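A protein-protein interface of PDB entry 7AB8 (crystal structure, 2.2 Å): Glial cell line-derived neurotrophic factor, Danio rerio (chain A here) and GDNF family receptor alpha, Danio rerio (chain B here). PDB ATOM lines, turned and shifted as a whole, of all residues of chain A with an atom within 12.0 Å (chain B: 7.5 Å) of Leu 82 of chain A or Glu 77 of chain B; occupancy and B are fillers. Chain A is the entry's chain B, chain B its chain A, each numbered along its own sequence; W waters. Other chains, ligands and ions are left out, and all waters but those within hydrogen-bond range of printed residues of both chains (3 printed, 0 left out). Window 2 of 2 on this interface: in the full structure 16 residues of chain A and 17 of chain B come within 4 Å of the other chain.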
ATOM      1  N   GLY A  20      25.965 -34.972  32.771  1.00  0.00           N
ATOM      2  CA  GLY A  20      25.622 -35.209  31.386  1.00  0.00           C
ATOM      3  C   GLY A  20      24.672 -34.202  30.774  1.00  0.00           C
ATOM      4  O   GLY A  20      24.504 -34.204  29.548  1.00  0.00           O
ATOM      5  N   TYR A  21      24.049 -33.349  31.581  1.00  0.00           N
ATOM      6  CA  TYR A  21      23.104 -32.377  31.050  1.00  0.00           C
ATOM      7  C   TYR A  21      23.834 -31.286  30.277  1.00  0.00           C
ATOM      8  O   TYR A  21      24.943 -30.880  30.636  1.00  0.00           O
ATOM      9  CB  TYR A  21      22.285 -31.760  32.183  1.00  0.00           C
ATOM     10  CG  TYR A  21      21.573 -32.784  33.037  1.00  0.00           C
ATOM     11  CD1 TYR A  21      20.436 -33.432  32.573  1.00  0.00           C
ATOM     12  CD2 TYR A  21      22.041 -33.107  34.304  1.00  0.00           C
ATOM     13  CE1 TYR A  21      19.783 -34.371  33.348  1.00  0.00           C
ATOM     14  CE2 TYR A  21      21.394 -34.044  35.086  1.00  0.00           C
ATOM     15  CZ  TYR A  21      20.265 -34.673  34.602  1.00  0.00           C
ATOM     16  OH  TYR A  21      19.616 -35.608  35.373  1.00  0.00           O
ATOM     17  N   ARG A  22      23.204 -30.815  29.205  1.00  0.00           N
ATOM     18  CA  ARG A  22      23.710 -29.700  28.410  1.00  0.00           C
ATOM     19  C   ARG A  22      22.737 -28.539  28.587  1.00  0.00           C
ATOM     20  O   ARG A  22      21.705 -28.471  27.913  1.00  0.00           O
ATOM     21  CB  ARG A  22      23.870 -30.092  26.944  1.00  0.00           C
ATOM     22  CG  ARG A  22      25.314 -30.054  26.462  1.00  0.00           C
ATOM     23  CD  ARG A  22      25.404 -30.178  24.951  1.00  0.00           C
ATOM     24  NE  ARG A  22      25.139 -28.909  24.281  1.00  0.00           N
ATOM     25  CZ  ARG A  22      24.140 -28.712  23.428  1.00  0.00           C
ATOM     26  NH1 ARG A  22      23.308 -29.703  23.139  1.00  0.00           N
ATOM     27  NH2 ARG A  22      23.973 -27.524  22.863  1.00  0.00           N
ATOM     28  N   THR A  23      23.071 -27.633  29.500  1.00  0.00           N
ATOM     29  CA  THR A  23      22.201 -26.517  29.839  1.00  0.00           C
ATOM     30  C   THR A  23      23.052 -25.397  30.414  1.00  0.00           C
ATOM     31  O   THR A  23      24.163 -25.626  30.900  1.00  0.00           O
ATOM     32  CB  THR A  23      21.117 -26.934  30.839  1.00  0.00           C
ATOM     33  OG1 THR A  23      20.471 -25.770  31.366  1.00  0.00           O
ATOM     34  CG2 THR A  23      21.731 -27.724  31.982  1.00  0.00           C
ATOM     35  N   LYS A  24      22.516 -24.182  30.356  1.00  0.00           N
ATOM     36  CA  LYS A  24      23.176 -23.017  30.926  1.00  0.00           C
ATOM     37  C   LYS A  24      22.556 -22.587  32.248  1.00  0.00           C
ATOM     38  O   LYS A  24      22.877 -21.504  32.750  1.00  0.00           O
ATOM     39  CB  LYS A  24      23.153 -21.857  29.928  1.00  0.00           C
ATOM     40  CG  LYS A  24      23.933 -22.130  28.652  1.00  0.00           C
ATOM     41  CD  LYS A  24      23.561 -21.150  27.552  1.00  0.00           C
ATOM     42  CE  LYS A  24      23.081 -21.876  26.304  1.00  0.00           C
ATOM     43  NZ  LYS A  24      24.210 -22.437  25.513  1.00  0.00           N
ATOM     44  N   GLU A  25      21.684 -23.409  32.824  1.00  0.00           N
ATOM     45  CA  GLU A  25      21.062 -23.087  34.097  1.00  0.00           C
ATOM     46  C   GLU A  25      22.053 -23.290  35.241  1.00  0.00           C
ATOM     47  O   GLU A  25      23.075 -23.968  35.103  1.00  0.00           O
ATOM     48  CB  GLU A  25      19.811 -23.940  34.311  1.00  0.00           C
ATOM     49  CG  GLU A  25      18.675 -23.612  33.350  1.00  0.00           C
ATOM     50  CD  GLU A  25      17.313 -23.632  34.018  1.00  0.00           C
ATOM     51  OE1 GLU A  25      17.253 -23.472  35.256  1.00  0.00           O
ATOM     52  OE2 GLU A  25      16.302 -23.811  33.306  1.00  0.00           O
ATOM     53  N   SER A  76      14.693 -28.103  39.264  1.00  0.00           N
ATOM     54  CA  SER A  76      14.385 -28.371  37.871  1.00  0.00           C
ATOM     55  C   SER A  76      15.141 -27.395  36.980  1.00  0.00           C
ATOM     56  O   SER A  76      15.576 -26.327  37.422  1.00  0.00           O
ATOM     57  CB  SER A  76      12.880 -28.262  37.607  1.00  0.00           C
ATOM     58  OG  SER A  76      12.184 -29.373  38.142  1.00  0.00           O
ATOM     59  N   PHE A  77      15.301 -27.776  35.715  1.00  0.00           N
ATOM     60  CA  PHE A  77      15.955 -26.914  34.741  1.00  0.00           C
ATOM     61  C   PHE A  77      15.614 -27.397  33.339  1.00  0.00           C
ATOM     62  O   PHE A  77      15.233 -28.552  33.133  1.00  0.00           O
ATOM     63  CB  PHE A  77      17.477 -26.871  34.948  1.00  0.00           C
ATOM     64  CG  PHE A  77      18.130 -28.224  34.979  1.00  0.00           C
ATOM     65  CD1 PHE A  77      18.511 -28.853  33.805  1.00  0.00           C
ATOM     66  CD2 PHE A  77      18.379 -28.860  36.184  1.00  0.00           C
ATOM     67  CE1 PHE A  77      19.116 -30.094  33.831  1.00  0.00           C
ATOM     68  CE2 PHE A  77      18.985 -30.102  36.218  1.00  0.00           C
ATOM     69  CZ  PHE A  77      19.354 -30.720  35.038  1.00  0.00           C
ATOM     70  N   LEU A  78      15.759 -26.489  32.379  1.00  0.00           N
ATOM     71  CA  LEU A  78      15.487 -26.753  30.973  1.00  0.00           C
ATOM     72  C   LEU A  78      16.807 -26.801  30.214  1.00  0.00           C
ATOM     73  O   LEU A  78      17.629 -25.888  30.341  1.00  0.00           O
ATOM     74  CB  LEU A  78      14.574 -25.672  30.392  1.00  0.00           C
ATOM     75  CG  LEU A  78      14.062 -25.832  28.962  1.00  0.00           C
ATOM     76  CD1 LEU A  78      12.954 -26.869  28.910  1.00  0.00           C
ATOM     77  CD2 LEU A  78      13.574 -24.494  28.424  1.00  0.00           C
ATOM     78  N   ASP A  79      17.013 -27.861  29.430  1.00  0.00           N
ATOM     79  CA  ASP A  79      18.272 -28.016  28.720  1.00  0.00           C
ATOM     80  C   ASP A  79      18.198 -27.350  27.345  1.00  0.00           C
ATOM     81  O   ASP A  79      17.176 -26.784  26.950  1.00  0.00           O
ATOM     82  CB  ASP A  79      18.668 -29.495  28.626  1.00  0.00           C
ATOM     83  CG  ASP A  79      17.730 -30.331  27.753  1.00  0.00           C
ATOM     84  OD1 ASP A  79      17.008 -29.791  26.889  1.00  0.00           O
ATOM     85  OD2 ASP A  79      17.729 -31.568  27.932  1.00  0.00           O
ATOM     86  N   ASP A  80      19.307 -27.429  26.602  1.00  0.00           N
ATOM     87  CA  ASP A  80      19.390 -26.766  25.305  1.00  0.00           C
ATOM     88  C   ASP A  80      18.416 -27.363  24.296  1.00  0.00           C
ATOM     89  O   ASP A  80      17.995 -26.669  23.363  1.00  0.00           O
ATOM     90  CB  ASP A  80      20.819 -26.844  24.770  1.00  0.00           C
ATOM     91  CG  ASP A  80      21.792 -26.014  25.585  1.00  0.00           C
ATOM     92  OD1 ASP A  80      21.357 -25.013  26.192  1.00  0.00           O
ATOM     93  OD2 ASP A  80      22.991 -26.363  25.619  1.00  0.00           O
ATOM     94  N   SER A  81      18.051 -28.632  24.458  1.00  0.00           N
ATOM     95  CA  SER A  81      17.085 -29.283  23.584  1.00  0.00           C
ATOM     96  C   SER A  81      15.646 -29.069  24.036  1.00  0.00           C
ATOM     97  O   SER A  81      14.749 -29.769  23.556  1.00  0.00           O
ATOM     98  CB  SER A  81      17.383 -30.782  23.494  1.00  0.00           C
ATOM     99  OG  SER A  81      18.779 -31.024  23.505  1.00  0.00           O
ATOM    100  N   LEU A  82      15.415 -28.126  24.954  1.00  0.00           N
ATOM    101  CA  LEU A  82      14.083 -27.765  25.434  1.00  0.00           C
ATOM    102  C   LEU A  82      13.396 -28.912  26.172  1.00  0.00           C
ATOM    103  O   LEU A  82      12.169 -29.025  26.149  1.00  0.00           O
ATOM    104  CB  LEU A  82      13.194 -27.260  24.292  1.00  0.00           C
ATOM    105  CG  LEU A  82      13.778 -26.114  23.465  1.00  0.00           C
ATOM    106  CD1 LEU A  82      12.930 -25.855  22.230  1.00  0.00           C
ATOM    107  CD2 LEU A  82      13.905 -24.858  24.313  1.00  0.00           C
ATOM    108  N   GLU A  83      14.171 -29.764  26.837  1.00  0.00           N
ATOM    109  CA  GLU A  83      13.635 -30.817  27.688  1.00  0.00           C
ATOM    110  C   GLU A  83      13.866 -30.459  29.150  1.00  0.00           C
ATOM    111  O   GLU A  83      14.955 -30.011  29.525  1.00  0.00           O
ATOM    112  CB  GLU A  83      14.279 -32.172  27.376  1.00  0.00           C
ATOM    113  CG  GLU A  83      14.183 -33.176  28.523  1.00  0.00           C
ATOM    114  CD  GLU A  83      14.460 -34.603  28.093  1.00  0.00           C
ATOM    115  OE1 GLU A  83      13.625 -35.485  28.383  1.00  0.00           O
ATOM    116  OE2 GLU A  83      15.515 -34.845  27.469  1.00  0.00           O
ATOM    117  N   TYR A  84      12.837 -30.654  29.970  1.00  0.00           N
ATOM    118  CA  TYR A  84      12.945 -30.397  31.399  1.00  0.00           C
ATOM    119  C   TYR A  84      13.529 -31.605  32.118  1.00  0.00           C
ATOM    120  O   TYR A  84      13.270 -32.753  31.747  1.00  0.00           O
ATOM    121  CB  TYR A  84      11.574 -30.062  31.989  1.00  0.00           C
ATOM    122  CG  TYR A  84      11.163 -28.615  31.843  1.00  0.00           C
ATOM    123  CD1 TYR A  84      11.842 -27.606  32.514  1.00  0.00           C
ATOM    124  CD2 TYR A  84      10.086 -28.258  31.042  1.00  0.00           C
ATOM    125  CE1 TYR A  84      11.465 -26.282  32.386  1.00  0.00           C
ATOM    126  CE2 TYR A  84       9.701 -26.937  30.908  1.00  0.00           C
ATOM    127  CZ  TYR A  84      10.393 -25.954  31.582  1.00  0.00           C
ATOM    128  OH  TYR A  84      10.011 -24.638  31.449  1.00  0.00           O
ATOM    129  N   HIS A  85      14.322 -31.337  33.153  1.00  0.00           N
ATOM    130  CA  HIS A  85      14.863 -32.370  34.022  1.00  0.00           C
ATOM    131  C   HIS A  85      14.681 -31.946  35.471  1.00  0.00           C
ATOM    132  O   HIS A  85      14.721 -30.756  35.793  1.00  0.00           O
ATOM    133  CB  HIS A  85      16.350 -32.636  33.745  1.00  0.00           C
ATOM    134  CG  HIS A  85      16.658 -32.944  32.313  1.00  0.00           C
ATOM    135  ND1 HIS A  85      16.657 -34.228  31.813  1.00  0.00           N
ATOM    136  CD2 HIS A  85      16.982 -32.137  31.276  1.00  0.00           C
ATOM    137  CE1 HIS A  85      16.965 -34.198  30.528  1.00  0.00           C
ATOM    138  NE2 HIS A  85      17.168 -32.941  30.178  1.00  0.00           N
ATOM    139  N   THR A  86      14.482 -32.930  36.343  1.00  0.00           N
ATOM    140  CA  THR A  86      14.320 -32.689  37.770  1.00  0.00           C
ATOM    141  C   THR A  86      15.279 -33.585  38.537  1.00  0.00           C
ATOM    142  O   THR A  86      15.334 -34.794  38.290  1.00  0.00           O
ATOM    143  CB  THR A  86      12.878 -32.948  38.224  1.00  0.00           C
ATOM    144  OG1 THR A  86      11.991 -32.043  37.554  1.00  0.00           O
ATOM    145  CG2 THR A  86      12.749 -32.754  39.729  1.00  0.00           C
ATOM    146  N   CYS B   4      15.355 -14.569  29.327  1.00  0.00           N
ATOM    147  CA  CYS B   4      14.625 -15.709  29.875  1.00  0.00           C
ATOM    148  C   CYS B   4      15.562 -16.657  30.613  1.00  0.00           C
ATOM    149  O   CYS B   4      15.184 -17.241  31.636  1.00  0.00           O
ATOM    150  CB  CYS B   4      13.882 -16.450  28.765  1.00  0.00           C
ATOM    151  SG  CYS B   4      12.672 -15.451  27.866  1.00  0.00           S
ATOM    152  N   CYS B  67      12.458 -11.180  24.539  1.00  0.00           N
ATOM    153  CA  CYS B  67      13.396 -11.757  23.594  1.00  0.00           C
ATOM    154  C   CYS B  67      13.361 -10.938  22.314  1.00  0.00           C
ATOM    155  O   CYS B  67      12.332 -10.327  21.985  1.00  0.00           O
ATOM    156  CB  CYS B  67      13.038 -13.216  23.277  1.00  0.00           C
ATOM    157  SG  CYS B  67      12.833 -14.203  24.746  1.00  0.00           S
ATOM    158  N   LEU B  69      13.791 -12.217  19.098  1.00  0.00           N
ATOM    159  CA  LEU B  69      13.018 -13.020  18.161  1.00  0.00           C
ATOM    160  C   LEU B  69      11.917 -13.757  18.911  1.00  0.00           C
ATOM    161  O   LEU B  69      12.166 -14.345  19.967  1.00  0.00           O
ATOM    162  CB  LEU B  69      13.915 -14.016  17.427  1.00  0.00           C
ATOM    163  CG  LEU B  69      15.015 -13.419  16.552  1.00  0.00           C
ATOM    164  CD1 LEU B  69      16.236 -14.325  16.529  1.00  0.00           C
ATOM    165  CD2 LEU B  69      14.489 -13.185  15.148  1.00  0.00           C
ATOM    166  N   GLY B  70      10.701 -13.723  18.362  1.00  0.00           N
ATOM    167  CA  GLY B  70       9.569 -14.392  18.970  1.00  0.00           C
ATOM    168  C   GLY B  70       9.399 -15.847  18.604  1.00  0.00           C
ATOM    169  O   GLY B  70       8.508 -16.512  19.139  1.00  0.00           O
ATOM    170  N   ASP B  71      10.231 -16.359  17.702  1.00  0.00           N
ATOM    171  CA  ASP B  71      10.180 -17.756  17.301  1.00  0.00           C
ATOM    172  C   ASP B  71      11.582 -18.200  16.914  1.00  0.00           C
ATOM    173  O   ASP B  71      12.415 -17.383  16.509  1.00  0.00           O
ATOM    174  CB  ASP B  71       9.201 -17.974  16.138  1.00  0.00           C
ATOM    175  CG  ASP B  71       8.995 -19.443  15.810  1.00  0.00           C
ATOM    176  OD1 ASP B  71       9.346 -20.299  16.650  1.00  0.00           O
ATOM    177  OD2 ASP B  71       8.480 -19.741  14.712  1.00  0.00           O
ATOM    178  N   GLN B  72      11.839 -19.503  17.077  1.00  0.00           N
ATOM    179  CA  GLN B  72      13.090 -20.156  16.700  1.00  0.00           C
ATOM    180  C   GLN B  72      14.259 -19.748  17.588  1.00  0.00           C
ATOM    181  O   GLN B  72      15.344 -20.333  17.501  1.00  0.00           O
ATOM    182  CB  GLN B  72      13.423 -19.880  15.230  1.00  0.00           C
ATOM    183  CG  GLN B  72      12.332 -20.291  14.245  1.00  0.00           C
ATOM    184  CD  GLN B  72      12.128 -21.799  14.151  1.00  0.00           C
ATOM    185  OE1 GLN B  72      11.962 -22.492  15.156  1.00  0.00           O
ATOM    186  NE2 GLN B  72      12.144 -22.312  12.928  1.00  0.00           N
ATOM    187  N   SER B  73      14.164 -18.683  18.374  1.00  0.00           N
ATOM    188  CA  SER B  73      15.318 -18.360  19.229  1.00  0.00           C
ATOM    189  C   SER B  73      15.305 -19.197  20.497  1.00  0.00           C
ATOM    190  O   SER B  73      14.321 -19.783  20.863  1.00  0.00           O
ATOM    191  CB  SER B  73      15.476 -16.882  19.556  1.00  0.00           C
ATOM    192  OG  SER B  73      14.378 -16.377  20.212  1.00  0.00           O
ATOM    193  N   ALA B  74      16.451 -19.254  21.122  1.00  0.00           N
ATOM    194  CA  ALA B  74      16.646 -19.979  22.375  1.00  0.00           C
ATOM    195  C   ALA B  74      15.899 -19.289  23.512  1.00  0.00           C
ATOM    196  O   ALA B  74      15.252 -19.949  24.334  1.00  0.00           O
ATOM    197  CB  ALA B  74      18.139 -20.092  22.692  1.00  0.00           C
ATOM    198  N   CYS B  75      16.011 -17.956  23.581  1.00  0.00           N
ATOM    199  CA  CYS B  75      15.128 -17.125  24.400  1.00  0.00           C
ATOM    200  C   CYS B  75      13.654 -17.482  24.236  1.00  0.00           C
ATOM    201  O   CYS B  75      12.973 -17.810  25.210  1.00  0.00           O
ATOM    202  CB  CYS B  75      15.311 -15.654  24.042  1.00  0.00           C
ATOM    203  SG  CYS B  75      14.741 -14.535  25.334  1.00  0.00           S
ATOM    204  N   SER B  76      13.125 -17.358  23.013  1.00  0.00           N
ATOM    205  CA  SER B  76      11.679 -17.438  22.831  1.00  0.00           C
ATOM    206  C   SER B  76      11.160 -18.846  23.046  1.00  0.00           C
ATOM    207  O   SER B  76      10.029 -19.016  23.512  1.00  0.00           O
ATOM    208  CB  SER B  76      11.306 -16.945  21.442  1.00  0.00           C
ATOM    209  OG  SER B  76      11.781 -17.840  20.452  1.00  0.00           O
ATOM    210  N   GLU B  77      11.953 -19.864  22.702  1.00  0.00           N
ATOM    211  CA  GLU B  77      11.530 -21.237  22.957  1.00  0.00           C
ATOM    212  C   GLU B  77      11.547 -21.544  24.449  1.00  0.00           C
ATOM    213  O   GLU B  77      10.682 -22.273  24.948  1.00  0.00           O
ATOM    214  CB  GLU B  77      12.419 -22.214  22.190  1.00  0.00           C
ATOM    215  CG  GLU B  77      12.207 -22.205  20.680  1.00  0.00           C
ATOM    216  CD  GLU B  77      10.748 -22.072  20.291  1.00  0.00           C
ATOM    217  OE1 GLU B  77      10.359 -20.990  19.803  1.00  0.00           O
ATOM    218  OE2 GLU B  77       9.991 -23.049  20.469  1.00  0.00           O
ATOM    219  N   ARG B  78      12.521 -20.996  25.180  1.00  0.00           N
ATOM    220  CA  ARG B  78      12.519 -21.143  26.632  1.00  0.00           C
ATOM    221  C   ARG B  78      11.301 -20.462  27.243  1.00  0.00           C
ATOM    222  O   ARG B  78      10.657 -21.014  28.143  1.00  0.00           O
ATOM    223  CB  ARG B  78      13.807 -20.572  27.223  1.00  0.00           C
ATOM    224  CG  ARG B  78      13.822 -20.521  28.746  1.00  0.00           C
ATOM    225  CD  ARG B  78      15.164 -20.042  29.278  1.00  0.00           C
ATOM    226  NE  ARG B  78      16.193 -21.077  29.197  1.00  0.00           N
ATOM    227  CZ  ARG B  78      16.399 -22.000  30.132  1.00  0.00           C
ATOM    228  NH1 ARG B  78      15.643 -22.021  31.222  1.00  0.00           N
ATOM    229  NH2 ARG B  78      17.359 -22.902  29.976  1.00  0.00           N
ATOM    230  N   ARG B  79      10.965 -19.263  26.759  1.00  0.00           N
ATOM    231  CA  ARG B  79       9.781 -18.566  27.249  1.00  0.00           C
ATOM    232  C   ARG B  79       8.514 -19.356  26.947  1.00  0.00           C
ATOM    233  O   ARG B  79       7.614 -19.448  27.792  1.00  0.00           O
ATOM    234  CB  ARG B  79       9.705 -17.171  26.628  1.00  0.00           C
ATOM    235  CG  ARG B  79       8.511 -16.347  27.080  1.00  0.00           C
ATOM    236  CD  ARG B  79       8.574 -14.936  26.513  1.00  0.00           C
ATOM    237  NE  ARG B  79       8.407 -14.922  25.062  1.00  0.00           N
ATOM    238  CZ  ARG B  79       8.725 -13.894  24.282  1.00  0.00           C
ATOM    239  NH1 ARG B  79       9.231 -12.788  24.812  1.00  0.00           N
ATOM    240  NH2 ARG B  79       8.538 -13.971  22.972  1.00  0.00           N
ATOM    241  N   ARG B  80       8.429 -19.939  25.748  1.00  0.00           N
ATOM    242  CA  ARG B  80       7.265 -20.743  25.391  1.00  0.00           C
ATOM    243  C   ARG B  80       7.145 -21.981  26.269  1.00  0.00           C
ATOM    244  O   ARG B  80       6.036 -22.477  26.495  1.00  0.00           O
ATOM    245  CB  ARG B  80       7.342 -21.143  23.917  1.00  0.00           C
ATOM    246  CG  ARG B  80       6.009 -21.530  23.300  1.00  0.00           C
ATOM    247  CD  ARG B  80       6.170 -21.958  21.845  1.00  0.00           C
ATOM    248  NE  ARG B  80       7.281 -21.276  21.183  1.00  0.00           N
ATOM    249  CZ  ARG B  80       7.220 -20.040  20.696  1.00  0.00           C
ATOM    250  NH1 ARG B  80       8.282 -19.503  20.111  1.00  0.00           N
ATOM    251  NH2 ARG B  80       6.100 -19.338  20.797  1.00  0.00           N
ATOM    252  N   GLN B  81       8.268 -22.489  26.774  1.00  0.00           N
ATOM    253  CA  GLN B  81       8.291 -23.686  27.605  1.00  0.00           C
ATOM    254  C   GLN B  81       8.026 -23.402  29.079  1.00  0.00           C
ATOM    255  O   GLN B  81       8.119 -24.327  29.894  1.00  0.00           O
ATOM    256  CB  GLN B  81       9.639 -24.397  27.457  1.00  0.00           C
ATOM    257  CG  GLN B  81       9.807 -25.164  26.158  1.00  0.00           C
ATOM    258  CD  GLN B  81       8.932 -26.400  26.098  1.00  0.00           C
ATOM    259  OE1 GLN B  81       7.902 -26.411  25.425  1.00  0.00           O
ATOM    260  NE2 GLN B  81       9.340 -27.450  26.801  1.00  0.00           N
ATOM    261  N   THR B  82       7.695 -22.157  29.438  1.00  0.00           N
ATOM    262  CA  THR B  82       7.565 -21.799  30.848  1.00  0.00           C
ATOM    263  C   THR B  82       6.439 -22.573  31.523  1.00  0.00           C
ATOM    264  O   THR B  82       6.588 -23.039  32.659  1.00  0.00           O
ATOM    265  CB  THR B  82       7.338 -20.293  30.993  1.00  0.00           C
ATOM    266  OG1 THR B  82       8.433 -19.582  30.403  1.00  0.00           O
ATOM    267  CG2 THR B  82       7.225 -19.911  32.463  1.00  0.00           C
ATOM    268  N   PRO B  85       4.063 -26.444  27.958  1.00  0.00           N
ATOM    269  CA  PRO B  85       2.846 -26.530  27.131  1.00  0.00           C
ATOM    270  C   PRO B  85       2.543 -27.924  26.612  1.00  0.00           C
ATOM    271  O   PRO B  85       1.374 -28.203  26.313  1.00  0.00           O
ATOM    272  CB  PRO B  85       3.137 -25.560  25.978  1.00  0.00           C
ATOM    273  CG  PRO B  85       4.623 -25.486  25.914  1.00  0.00           C
ATOM    274  CD  PRO B  85       5.096 -25.602  27.332  1.00  0.00           C
ATOM    275  N   LEU B 156       2.323 -17.694  20.978  1.00  0.00           N
ATOM    276  CA  LEU B 156       2.286 -18.324  19.671  1.00  0.00           C
ATOM    277  C   LEU B 156       3.618 -18.130  18.954  1.00  0.00           C
ATOM    278  O   LEU B 156       4.417 -17.252  19.294  1.00  0.00           O
ATOM    279  CB  LEU B 156       1.147 -17.750  18.828  1.00  0.00           C
ATOM    280  CG  LEU B 156      -0.257 -17.853  19.426  1.00  0.00           C
ATOM    281  CD1 LEU B 156      -1.282 -17.213  18.503  1.00  0.00           C
ATOM    282  CD2 LEU B 156      -0.614 -19.304  19.703  1.00  0.00           C
ATOM    283  N   ARG B 157       3.854 -18.970  17.950  1.00  0.00           N
ATOM    284  CA  ARG B 157       5.057 -18.867  17.124  1.00  0.00           C
ATOM    285  C   ARG B 157       4.827 -17.758  16.105  1.00  0.00           C
ATOM    286  O   ARG B 157       4.299 -17.977  15.014  1.00  0.00           O
ATOM    287  CB  ARG B 157       5.373 -20.200  16.461  1.00  0.00           C
ATOM    288  CG  ARG B 157       5.763 -21.276  17.457  1.00  0.00           C
ATOM    289  CD  ARG B 157       5.911 -22.636  16.801  1.00  0.00           C
ATOM    290  NE  ARG B 157       6.202 -23.668  17.790  1.00  0.00           N
ATOM    291  CZ  ARG B 157       7.409 -23.899  18.295  1.00  0.00           C
ATOM    292  NH1 ARG B 157       7.579 -24.859  19.194  1.00  0.00           N
ATOM    293  NH2 ARG B 157       8.446 -23.172  17.901  1.00  0.00           N
HETATM  294  O   HOH W   1      17.371 -24.130  26.905  1.00  0.00           O
HETATM  295  O   HOH W   2      20.061 -24.278  28.463  1.00  0.00           O
HETATM  296  O   HOH W   3      11.114 -22.456  30.472  1.00  0.00           O
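Among the printed residues, merely in contact across the chains: Leu 82 of chain A with Glu 77 of chain B (3.7 Å) and Tyr 84 of chain A with Thr 82 of chain B (3.8 Å).
Water W3 lies within hydrogen-bond range of OH of Tyr 84 of chain A (2.6 Å) and O of Arg 78 of chain B (2.8 Å). Water W1 lies within hydrogen-bond range of O of Asp 79 of chain A and NH2 of Arg 78 of chain B. Water W2 lies within hydrogen-bond range of OD1 of Asp 80 of chain A (2.7 Å), N of Lys 24 of chain A (3.1 Å), OG1 of Thr 23 of chain A (3.3 Å), NH2 of Arg 78 of chain B (3.4 Å) and O of Leu 78 of chain A (3.5 Å).
Of the printed residues of chain B, Glu 25 of chain A touches Arg 78. Of the printed residues of chain B, Leu 78 of chain A touches Arg 78 (3.0 Å). Of chain B, only Glu 77 (3.7 Å) and Gln 81 (3.3 Å) come within 4 Å of Leu 82 of chain A. Of the printed residues of chain B, Tyr 84 of chain A touches Gln 81 (2.5 Å) and Thr 82 (3.8 Å). His 85 of chain A touches none of the printed residues of chain B. No residue of chain A comes within 4 Å of Gly 70 of chain B. No residue of chain A comes within 4 Å of Asp 71 of chain B. No residue of chain A comes within 4 Å of Gln 72 of chain B. No residue of chain A comes within 4 Å of Ser 73 of chain B. No residue of chain A comes within 4 Å of Ala 74 of chain B. No residue of chain A comes within 4 Å of Cys 75 of chain B. Glu 77 of chain B touches just one residue of chain A: Leu 82 (3.7 Å). No residue of chain A comes within 4 Å of Arg 80 of chain B. Printed residues of chain A within 4 Å of Thr 82 of chain B: Tyr 84. The nearest residue of chain B that does not touch Leu 82 of chain A is Arg 78 of chain B (4.2 Å).
NH1 of Arg 78 of chain B is in salt-bridge range of OE2 of Glu 25 of chain A, 2.8 Å away. The guanidinium group of Arg 78 of chain B is in hydrogen-bond range of the backbone carbonyl oxygen of Leu 78 of chain A (3.0 Å). NE2 of Gln 81 of chain B lies within hydrogen-bond range of O of Leu 82 of chain A (3.3 Å). OH of Tyr 84 of chain A lies within hydrogen-bond range of O of Gln 81 of chain B, at 2.5 Å.
Of the 19 printed residues of chain B, 4 touch a printed residue of chain A. Among the printed residues, Asp or Glu carboxylates within 4 Å of a Lys or Arg side-chain nitrogen of the other chain: Glu 25 of chain A with Arg 78 of chain B (2.8 Å).
The side-chain carboxylate (OE1) of Glu 77 of chain B sits at hydrogen-bond distance from the backbone NH (N) of Gln 72 of chain B (3.4 Å). OE1 of Glu 77 of chain B is in salt-bridge range of NH1 of Arg 80 of chain B, at 2.6 Å. The side-chain carboxylate (OE2) of Glu 77 of chain B is in salt-bridge range of the guanidinium group (NH2) of Arg 157 of chain B, at 3.0 Å. The side-chain hydroxyl (OG1) of Thr 23 of chain A is in hydrogen-bond range of the backbone NH (N) of Glu 25 of chain A (3.0 Å). The side-chain carboxylate (OD1) of Asp 79 of chain A is in hydrogen-bond range of the backbone NH (N) of Leu 82 of chain A, 3.0 Å away. SG of Cys 67 of chain B forms a disulfide with SG of Cys 75 of chain B, 2.0 Å away.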
